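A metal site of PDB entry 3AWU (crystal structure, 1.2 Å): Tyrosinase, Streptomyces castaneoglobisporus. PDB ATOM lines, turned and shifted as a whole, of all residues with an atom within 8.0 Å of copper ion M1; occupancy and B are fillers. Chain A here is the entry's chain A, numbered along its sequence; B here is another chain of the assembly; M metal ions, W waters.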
ATOM      1  N   HIS A  38      -4.311  24.162  -8.633  1.00  0.00           N
ATOM      2  CA  HIS A  38      -4.202  24.819  -7.345  1.00  0.00           C
ATOM      3  C   HIS A  38      -2.973  25.719  -7.255  1.00  0.00           C
ATOM      4  O   HIS A  38      -3.056  26.844  -6.760  1.00  0.00           O
ATOM      5  CB  HIS A  38      -4.105  23.696  -6.258  1.00  0.00           C
ATOM      6  CG  HIS A  38      -4.231  24.310  -4.891  1.00  0.00           C
ATOM      7  ND1 HIS A  38      -3.165  24.588  -4.089  1.00  0.00           N
ATOM      8  CD2 HIS A  38      -5.317  24.663  -4.186  1.00  0.00           C
ATOM      9  CE1 HIS A  38      -3.561  25.107  -2.929  1.00  0.00           C
ATOM     10  NE2 HIS A  38      -4.871  25.149  -2.984  1.00  0.00           N
ATOM     11  N   ILE A  42      -2.798  29.696  -6.228  1.00  0.00           N
ATOM     12  CA  ILE A  42      -2.138  30.190  -5.008  1.00  0.00           C
ATOM     13  C   ILE A  42      -0.986  31.088  -5.356  1.00  0.00           C
ATOM     14  O   ILE A  42      -0.647  32.012  -4.586  1.00  0.00           O
ATOM     15  CB  ILE A  42      -1.730  28.930  -4.192  1.00  0.00           C
ATOM     16  CG1 ILE A  42      -1.684  29.260  -2.698  1.00  0.00           C
ATOM     17  CG2 ILE A  42      -0.462  28.400  -4.747  1.00  0.00           C
ATOM     18  CD1 ILE A  42      -1.602  27.958  -1.925  1.00  0.00           C
ATOM     19  N   GLY A  53      -8.945  32.078  -5.298  1.00  0.00           N
ATOM     20  CA  GLY A  53      -8.898  30.789  -4.621  1.00  0.00           C
ATOM     21  C   GLY A  53      -8.579  30.901  -3.140  1.00  0.00           C
ATOM     22  O   GLY A  53      -8.944  30.019  -2.355  1.00  0.00           O
ATOM     23  N   HIS A  54      -7.858  31.933  -2.758  1.00  0.00           N
ATOM     24  CA  HIS A  54      -7.239  32.150  -1.453  1.00  0.00           C
ATOM     25  C   HIS A  54      -7.405  33.610  -1.052  1.00  0.00           C
ATOM     26  O   HIS A  54      -7.694  34.471  -1.884  1.00  0.00           O
ATOM     27  CB  HIS A  54      -5.722  31.807  -1.492  1.00  0.00           C
ATOM     28  CG  HIS A  54      -5.540  30.388  -1.959  1.00  0.00           C
ATOM     29  ND1 HIS A  54      -5.457  30.009  -3.272  1.00  0.00           N
ATOM     30  CD2 HIS A  54      -5.505  29.235  -1.220  1.00  0.00           C
ATOM     31  CE1 HIS A  54      -5.334  28.683  -3.300  1.00  0.00           C
ATOM     32  NE2 HIS A  54      -5.357  28.167  -2.087  1.00  0.00           N
ATOM     33  N   PHE A  59     -12.386  32.015  -1.041  1.00  0.00           N
ATOM     34  CA  PHE A  59     -11.588  30.897  -0.535  1.00  0.00           C
ATOM     35  C   PHE A  59     -12.483  29.688  -0.263  1.00  0.00           C
ATOM     36  O   PHE A  59     -12.161  28.553  -0.695  1.00  0.00           O
ATOM     37  CB  PHE A  59     -10.872  31.313   0.731  1.00  0.00           C
ATOM     38  CG  PHE A  59     -10.239  30.180   1.555  1.00  0.00           C
ATOM     39  CD1 PHE A  59      -9.170  29.454   1.051  1.00  0.00           C
ATOM     40  CD2 PHE A  59     -10.701  29.896   2.835  1.00  0.00           C
ATOM     41  CE1 PHE A  59      -8.567  28.472   1.818  1.00  0.00           C
ATOM     42  CE2 PHE A  59     -10.137  28.890   3.597  1.00  0.00           C
ATOM     43  CZ  PHE A  59      -9.070  28.186   3.077  1.00  0.00           C
ATOM     44  N   HIS A  63     -12.761  26.477  -2.899  1.00  0.00           N
ATOM     45  CA  HIS A  63     -12.304  25.130  -2.502  1.00  0.00           C
ATOM     46  C   HIS A  63     -13.453  24.149  -2.448  1.00  0.00           C
ATOM     47  O   HIS A  63     -13.251  22.958  -2.701  1.00  0.00           O
ATOM     48  CB  HIS A  63     -11.589  25.188  -1.144  1.00  0.00           C
ATOM     49  CG  HIS A  63     -10.158  25.674  -1.319  1.00  0.00           C
ATOM     50  ND1 HIS A  63      -9.791  27.020  -1.384  1.00  0.00           N
ATOM     51  CD2 HIS A  63      -8.993  24.997  -1.544  1.00  0.00           C
ATOM     52  CE1 HIS A  63      -8.465  27.127  -1.590  1.00  0.00           C
ATOM     53  NE2 HIS A  63      -7.933  25.903  -1.677  1.00  0.00           N
ATOM     54  N   GLU A 182      -9.332  30.684   7.463  1.00  0.00           N
ATOM     55  CA  GLU A 182      -8.197  30.499   6.566  1.00  0.00           C
ATOM     56  C   GLU A 182      -6.874  30.537   7.316  1.00  0.00           C
ATOM     57  O   GLU A 182      -5.984  29.718   7.159  1.00  0.00           O
ATOM     58  CB  GLU A 182      -8.282  31.564   5.450  1.00  0.00           C
ATOM     59  CG  GLU A 182      -7.250  31.279   4.337  1.00  0.00           C
ATOM     60  CD  GLU A 182      -7.356  32.209   3.151  1.00  0.00           C
ATOM     61  OE1 GLU A 182      -8.303  33.037   3.046  1.00  0.00           O
ATOM     62  OE2 GLU A 182      -6.476  32.076   2.272  1.00  0.00           O
ATOM     63  N   HIS A 190      -6.665  26.914   9.220  1.00  0.00           N
ATOM     64  CA  HIS A 190      -6.282  26.175   8.019  1.00  0.00           C
ATOM     65  C   HIS A 190      -4.837  26.297   7.638  1.00  0.00           C
ATOM     66  O   HIS A 190      -4.216  25.323   7.218  1.00  0.00           O
ATOM     67  CB  HIS A 190      -7.223  26.653   6.854  1.00  0.00           C
ATOM     68  CG  HIS A 190      -6.640  26.589   5.483  1.00  0.00           C
ATOM     69  ND1 HIS A 190      -5.840  27.605   4.978  1.00  0.00           N
ATOM     70  CD2 HIS A 190      -6.724  25.663   4.506  1.00  0.00           C
ATOM     71  CE1 HIS A 190      -5.470  27.287   3.724  1.00  0.00           C
ATOM     72  NE2 HIS A 190      -5.966  26.122   3.431  1.00  0.00           N
ATOM     73  N   ASN A 191      -4.252  27.518   7.719  1.00  0.00           N
ATOM     74  CA  ASN A 191      -2.835  27.663   7.301  1.00  0.00           C
ATOM     75  C   ASN A 191      -1.937  26.847   8.227  1.00  0.00           C
ATOM     76  O   ASN A 191      -0.996  26.185   7.747  1.00  0.00           O
ATOM     77  CB  ASN A 191      -2.414  29.120   7.318  1.00  0.00           C
ATOM     78  CG  ASN A 191      -2.929  29.953   6.175  1.00  0.00           C
ATOM     79  OD1 ASN A 191      -3.590  29.489   5.238  1.00  0.00           O
ATOM     80  ND2 ASN A 191      -2.692  31.265   6.284  1.00  0.00           N
ATOM     81  N   VAL A 193      -2.555  24.082   9.763  1.00  0.00           N
ATOM     82  CA  VAL A 193      -2.537  22.658   9.466  1.00  0.00           C
ATOM     83  C   VAL A 193      -1.587  22.346   8.291  1.00  0.00           C
ATOM     84  O   VAL A 193      -0.853  21.350   8.333  1.00  0.00           O
ATOM     85  CB  VAL A 193      -3.954  22.177   9.156  1.00  0.00           C
ATOM     86  CG1 VAL A 193      -3.967  20.684   8.726  1.00  0.00           C
ATOM     87  CG2 VAL A 193      -4.896  22.327  10.353  1.00  0.00           C
ATOM     88  N   HIS A 194      -1.595  23.186   7.235  1.00  0.00           N
ATOM     89  CA  HIS A 194      -0.642  23.013   6.159  1.00  0.00           C
ATOM     90  C   HIS A 194       0.816  23.007   6.680  1.00  0.00           C
ATOM     91  O   HIS A 194       1.630  22.170   6.341  1.00  0.00           O
ATOM     92  CB  HIS A 194      -0.747  24.088   5.081  1.00  0.00           C
ATOM     93  CG  HIS A 194      -1.869  23.953   4.095  1.00  0.00           C
ATOM     94  ND1 HIS A 194      -1.688  23.164   2.961  1.00  0.00           N
ATOM     95  CD2 HIS A 194      -3.080  24.521   3.997  1.00  0.00           C
ATOM     96  CE1 HIS A 194      -2.815  23.278   2.244  1.00  0.00           C
ATOM     97  NE2 HIS A 194      -3.697  24.088   2.830  1.00  0.00           N
ATOM     98  N   MET A 201       2.739  19.597   1.468  1.00  0.00           N
ATOM     99  CA  MET A 201       1.543  20.255   2.032  1.00  0.00           C
ATOM    100  C   MET A 201       1.833  21.655   2.496  1.00  0.00           C
ATOM    101  O   MET A 201       0.872  22.450   2.616  1.00  0.00           O
ATOM    102  CB  MET A 201       1.053  19.400   3.176  1.00  0.00           C
ATOM    103  CG  MET A 201      -0.233  18.830   3.206  1.00  0.00           C
ATOM    104  SD  MET A 201      -1.676  19.499   2.455  1.00  0.00           S
ATOM    105  CE  MET A 201      -2.725  19.981   3.824  1.00  0.00           C
ATOM    106  N   THR A 203       3.593  23.837   0.811  1.00  0.00           N
ATOM    107  CA  THR A 203       4.040  24.532  -0.375  1.00  0.00           C
ATOM    108  C   THR A 203       2.876  24.872  -1.309  1.00  0.00           C
ATOM    109  O   THR A 203       1.743  24.456  -1.067  1.00  0.00           O
ATOM    110  CB  THR A 203       5.068  23.746  -1.187  1.00  0.00           C
ATOM    111  OG1 THR A 203       4.369  22.690  -1.915  1.00  0.00           O
ATOM    112  CG2 THR A 203       6.133  23.145  -0.307  1.00  0.00           C
ATOM    113  N   SER A 206       0.568  21.878  -2.706  1.00  0.00           N
ATOM    114  CA  SER A 206       0.107  21.079  -1.573  1.00  0.00           C
ATOM    115  C   SER A 206      -0.854  19.965  -1.962  1.00  0.00           C
ATOM    116  O   SER A 206      -0.819  18.957  -1.231  1.00  0.00           O
ATOM    117  CB  SER A 206      -0.520  22.016  -0.515  1.00  0.00           C
ATOM    118  OG  SER A 206      -1.548  22.819  -1.053  1.00  0.00           O
ATOM    119  N   PRO A 207      -1.635  19.974  -3.029  1.00  0.00           N
ATOM    120  CA  PRO A 207      -2.438  18.786  -3.376  1.00  0.00           C
ATOM    121  C   PRO A 207      -1.587  17.595  -3.770  1.00  0.00           C
ATOM    122  O   PRO A 207      -2.148  16.501  -3.967  1.00  0.00           O
ATOM    123  CB  PRO A 207      -3.371  19.237  -4.519  1.00  0.00           C
ATOM    124  CG  PRO A 207      -3.453  20.723  -4.309  1.00  0.00           C
ATOM    125  CD  PRO A 207      -2.068  21.135  -3.878  1.00  0.00           C
ATOM    126  N   PHE A 212      -4.318  16.696   1.563  1.00  0.00           N
ATOM    127  CA  PHE A 212      -4.902  17.966   1.182  1.00  0.00           C
ATOM    128  C   PHE A 212      -6.417  17.921   1.145  1.00  0.00           C
ATOM    129  O   PHE A 212      -7.088  18.825   1.594  1.00  0.00           O
ATOM    130  CB  PHE A 212      -4.326  18.350  -0.210  1.00  0.00           C
ATOM    131  CG  PHE A 212      -4.935  19.603  -0.787  1.00  0.00           C
ATOM    132  CD1 PHE A 212      -6.086  19.553  -1.577  1.00  0.00           C
ATOM    133  CD2 PHE A 212      -4.328  20.823  -0.523  1.00  0.00           C
ATOM    134  CE1 PHE A 212      -6.677  20.713  -2.068  1.00  0.00           C
ATOM    135  CE2 PHE A 212      -4.881  21.982  -1.029  1.00  0.00           C
ATOM    136  CZ  PHE A 212      -6.073  21.951  -1.804  1.00  0.00           C
ATOM    137  N   HIS A 215      -8.021  17.529   4.649  1.00  0.00           N
ATOM    138  CA  HIS A 215      -7.965  18.807   5.355  1.00  0.00           C
ATOM    139  C   HIS A 215      -9.020  19.751   4.805  1.00  0.00           C
ATOM    140  O   HIS A 215      -9.838  20.332   5.565  1.00  0.00           O
ATOM    141  CB  HIS A 215      -6.555  19.385   5.118  1.00  0.00           C
ATOM    142  CG  HIS A 215      -6.393  20.786   5.627  1.00  0.00           C
ATOM    143  ND1 HIS A 215      -6.970  21.215   6.787  1.00  0.00           N
ATOM    144  CD2 HIS A 215      -5.634  21.815   5.154  1.00  0.00           C
ATOM    145  CE1 HIS A 215      -6.606  22.441   7.030  1.00  0.00           C
ATOM    146  NE2 HIS A 215      -5.820  22.867   6.061  1.00  0.00           N
ATOM    147  N   HIS A 216      -9.056  19.938   3.483  1.00  0.00           N
ATOM    148  CA  HIS A 216     -10.033  20.882   2.939  1.00  0.00           C
ATOM    149  C   HIS A 216     -11.441  20.389   3.112  1.00  0.00           C
ATOM    150  O   HIS A 216     -12.363  21.234   3.202  1.00  0.00           O
ATOM    151  CB  HIS A 216      -9.711  21.260   1.454  1.00  0.00           C
ATOM    152  CG  HIS A 216      -8.777  22.423   1.455  1.00  0.00           C
ATOM    153  ND1 HIS A 216      -9.283  23.722   1.593  1.00  0.00           N
ATOM    154  CD2 HIS A 216      -7.428  22.551   1.392  1.00  0.00           C
ATOM    155  CE1 HIS A 216      -8.258  24.548   1.615  1.00  0.00           C
ATOM    156  NE2 HIS A 216      -7.112  23.879   1.481  1.00  0.00           N
ATOM    157  N   VAL A 219     -12.208  21.784   6.532  1.00  0.00           N
ATOM    158  CA  VAL A 219     -12.427  23.231   6.433  1.00  0.00           C
ATOM    159  C   VAL A 219     -13.814  23.519   5.868  1.00  0.00           C
ATOM    160  O   VAL A 219     -14.526  24.406   6.321  1.00  0.00           O
ATOM    161  CB  VAL A 219     -11.298  23.835   5.564  1.00  0.00           C
ATOM    162  CG1 VAL A 219     -11.541  25.316   5.256  1.00  0.00           C
ATOM    163  CG2 VAL A 219      -9.935  23.670   6.234  1.00  0.00           C
ATOM    164  N   HIS B  97       4.283  28.541   1.675  1.00  0.00           N
ATOM    165  CA  HIS B  97       3.252  29.485   1.285  1.00  0.00           C
ATOM    166  C   HIS B  97       2.311  29.825   2.415  1.00  0.00           C
ATOM    167  O   HIS B  97       1.553  30.802   2.292  1.00  0.00           O
ATOM    168  CB  HIS B  97       2.446  28.792   0.155  1.00  0.00           C
ATOM    169  CG  HIS B  97       1.451  29.796  -0.311  1.00  0.00           C
ATOM    170  ND1 HIS B  97       1.741  30.785  -1.207  1.00  0.00           N
ATOM    171  CD2 HIS B  97       0.144  29.982  -0.028  1.00  0.00           C
ATOM    172  CE1 HIS B  97       0.678  31.526  -1.439  1.00  0.00           C
ATOM    173  NE2 HIS B  97      -0.323  31.068  -0.739  1.00  0.00           N
ATOM    174  N   TYR B  98       2.277  29.050   3.489  1.00  0.00           N
ATOM    175  CA  TYR B  98       1.237  29.231   4.501  1.00  0.00           C
ATOM    176  C   TYR B  98       1.841  29.755   5.787  1.00  0.00           C
ATOM    177  O   TYR B  98       1.182  29.723   6.830  1.00  0.00           O
ATOM    178  CB  TYR B  98       0.567  27.870   4.709  1.00  0.00           C
ATOM    179  CG  TYR B  98      -0.135  27.335   3.473  1.00  0.00           C
ATOM    180  CD1 TYR B  98       0.537  26.388   2.713  1.00  0.00           C
ATOM    181  CD2 TYR B  98      -1.417  27.710   3.071  1.00  0.00           C
ATOM    182  CE1 TYR B  98      -0.037  25.845   1.562  1.00  0.00           C
ATOM    183  CE2 TYR B  98      -1.997  27.149   1.932  1.00  0.00           C
ATOM    184  CZ  TYR B  98      -1.312  26.204   1.174  1.00  0.00           C
ATOM    185  OH  TYR B  98      -1.889  25.673   0.039  1.00  0.00           O
HETATM  186 CU    CU M   1      -5.315  24.968   1.891  1.00  0.00          CU
HETATM  187 CU    CU M   2      -5.270  26.367  -1.218  1.00  0.00          CU
HETATM  188  O   HOH W   1      -5.426  27.257   0.788  1.00  0.00           O
HETATM  189  O   HOH W   2      -4.701  25.206   0.121  1.00  0.00           O
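Copper ion M1 is bound by water W2, 1.9 Å away. A ring nitrogen (NE2) of His 190 binds copper ion M1, 2.0 Å away. Copper ion M1 is bound by a ring nitrogen (NE2) of His 194 (2.1 Å). Copper ion M1 is bound by NE2 of His 216, at 2.1 Å. Copper ion M1 is bound by water W1 (2.5 Å). Copper ion M1 has five donor atoms within binding distance.
A ring nitrogen (ND1) of His 190 sits at hydrogen-bond distance from the backbone carbonyl oxygen (O) of Glu 182 (3.0 Å). The side-chain amide oxygen (OD1) of Asn 191 sits at hydrogen-bond distance from a ring nitrogen (ND1) of His 190, at 2.9 Å. NE2 of His 215 is in hydrogen-bond range of O of His 190. OH of Tyr 98 of chain B is in hydrogen-bond range of OG of Ser 206 (3.1 Å). The backbone carbonyl oxygen (O) of Met 201 is in hydrogen-bond range of a ring nitrogen (ND1) of His 194, at 2.7 Å.
OH of Tyr 98 of chain B touches copper ion M1, 3.96 Å away. Within 4 Å of copper ion M1: His 190, His 194, His 216 and Tyr 98 of chain B.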
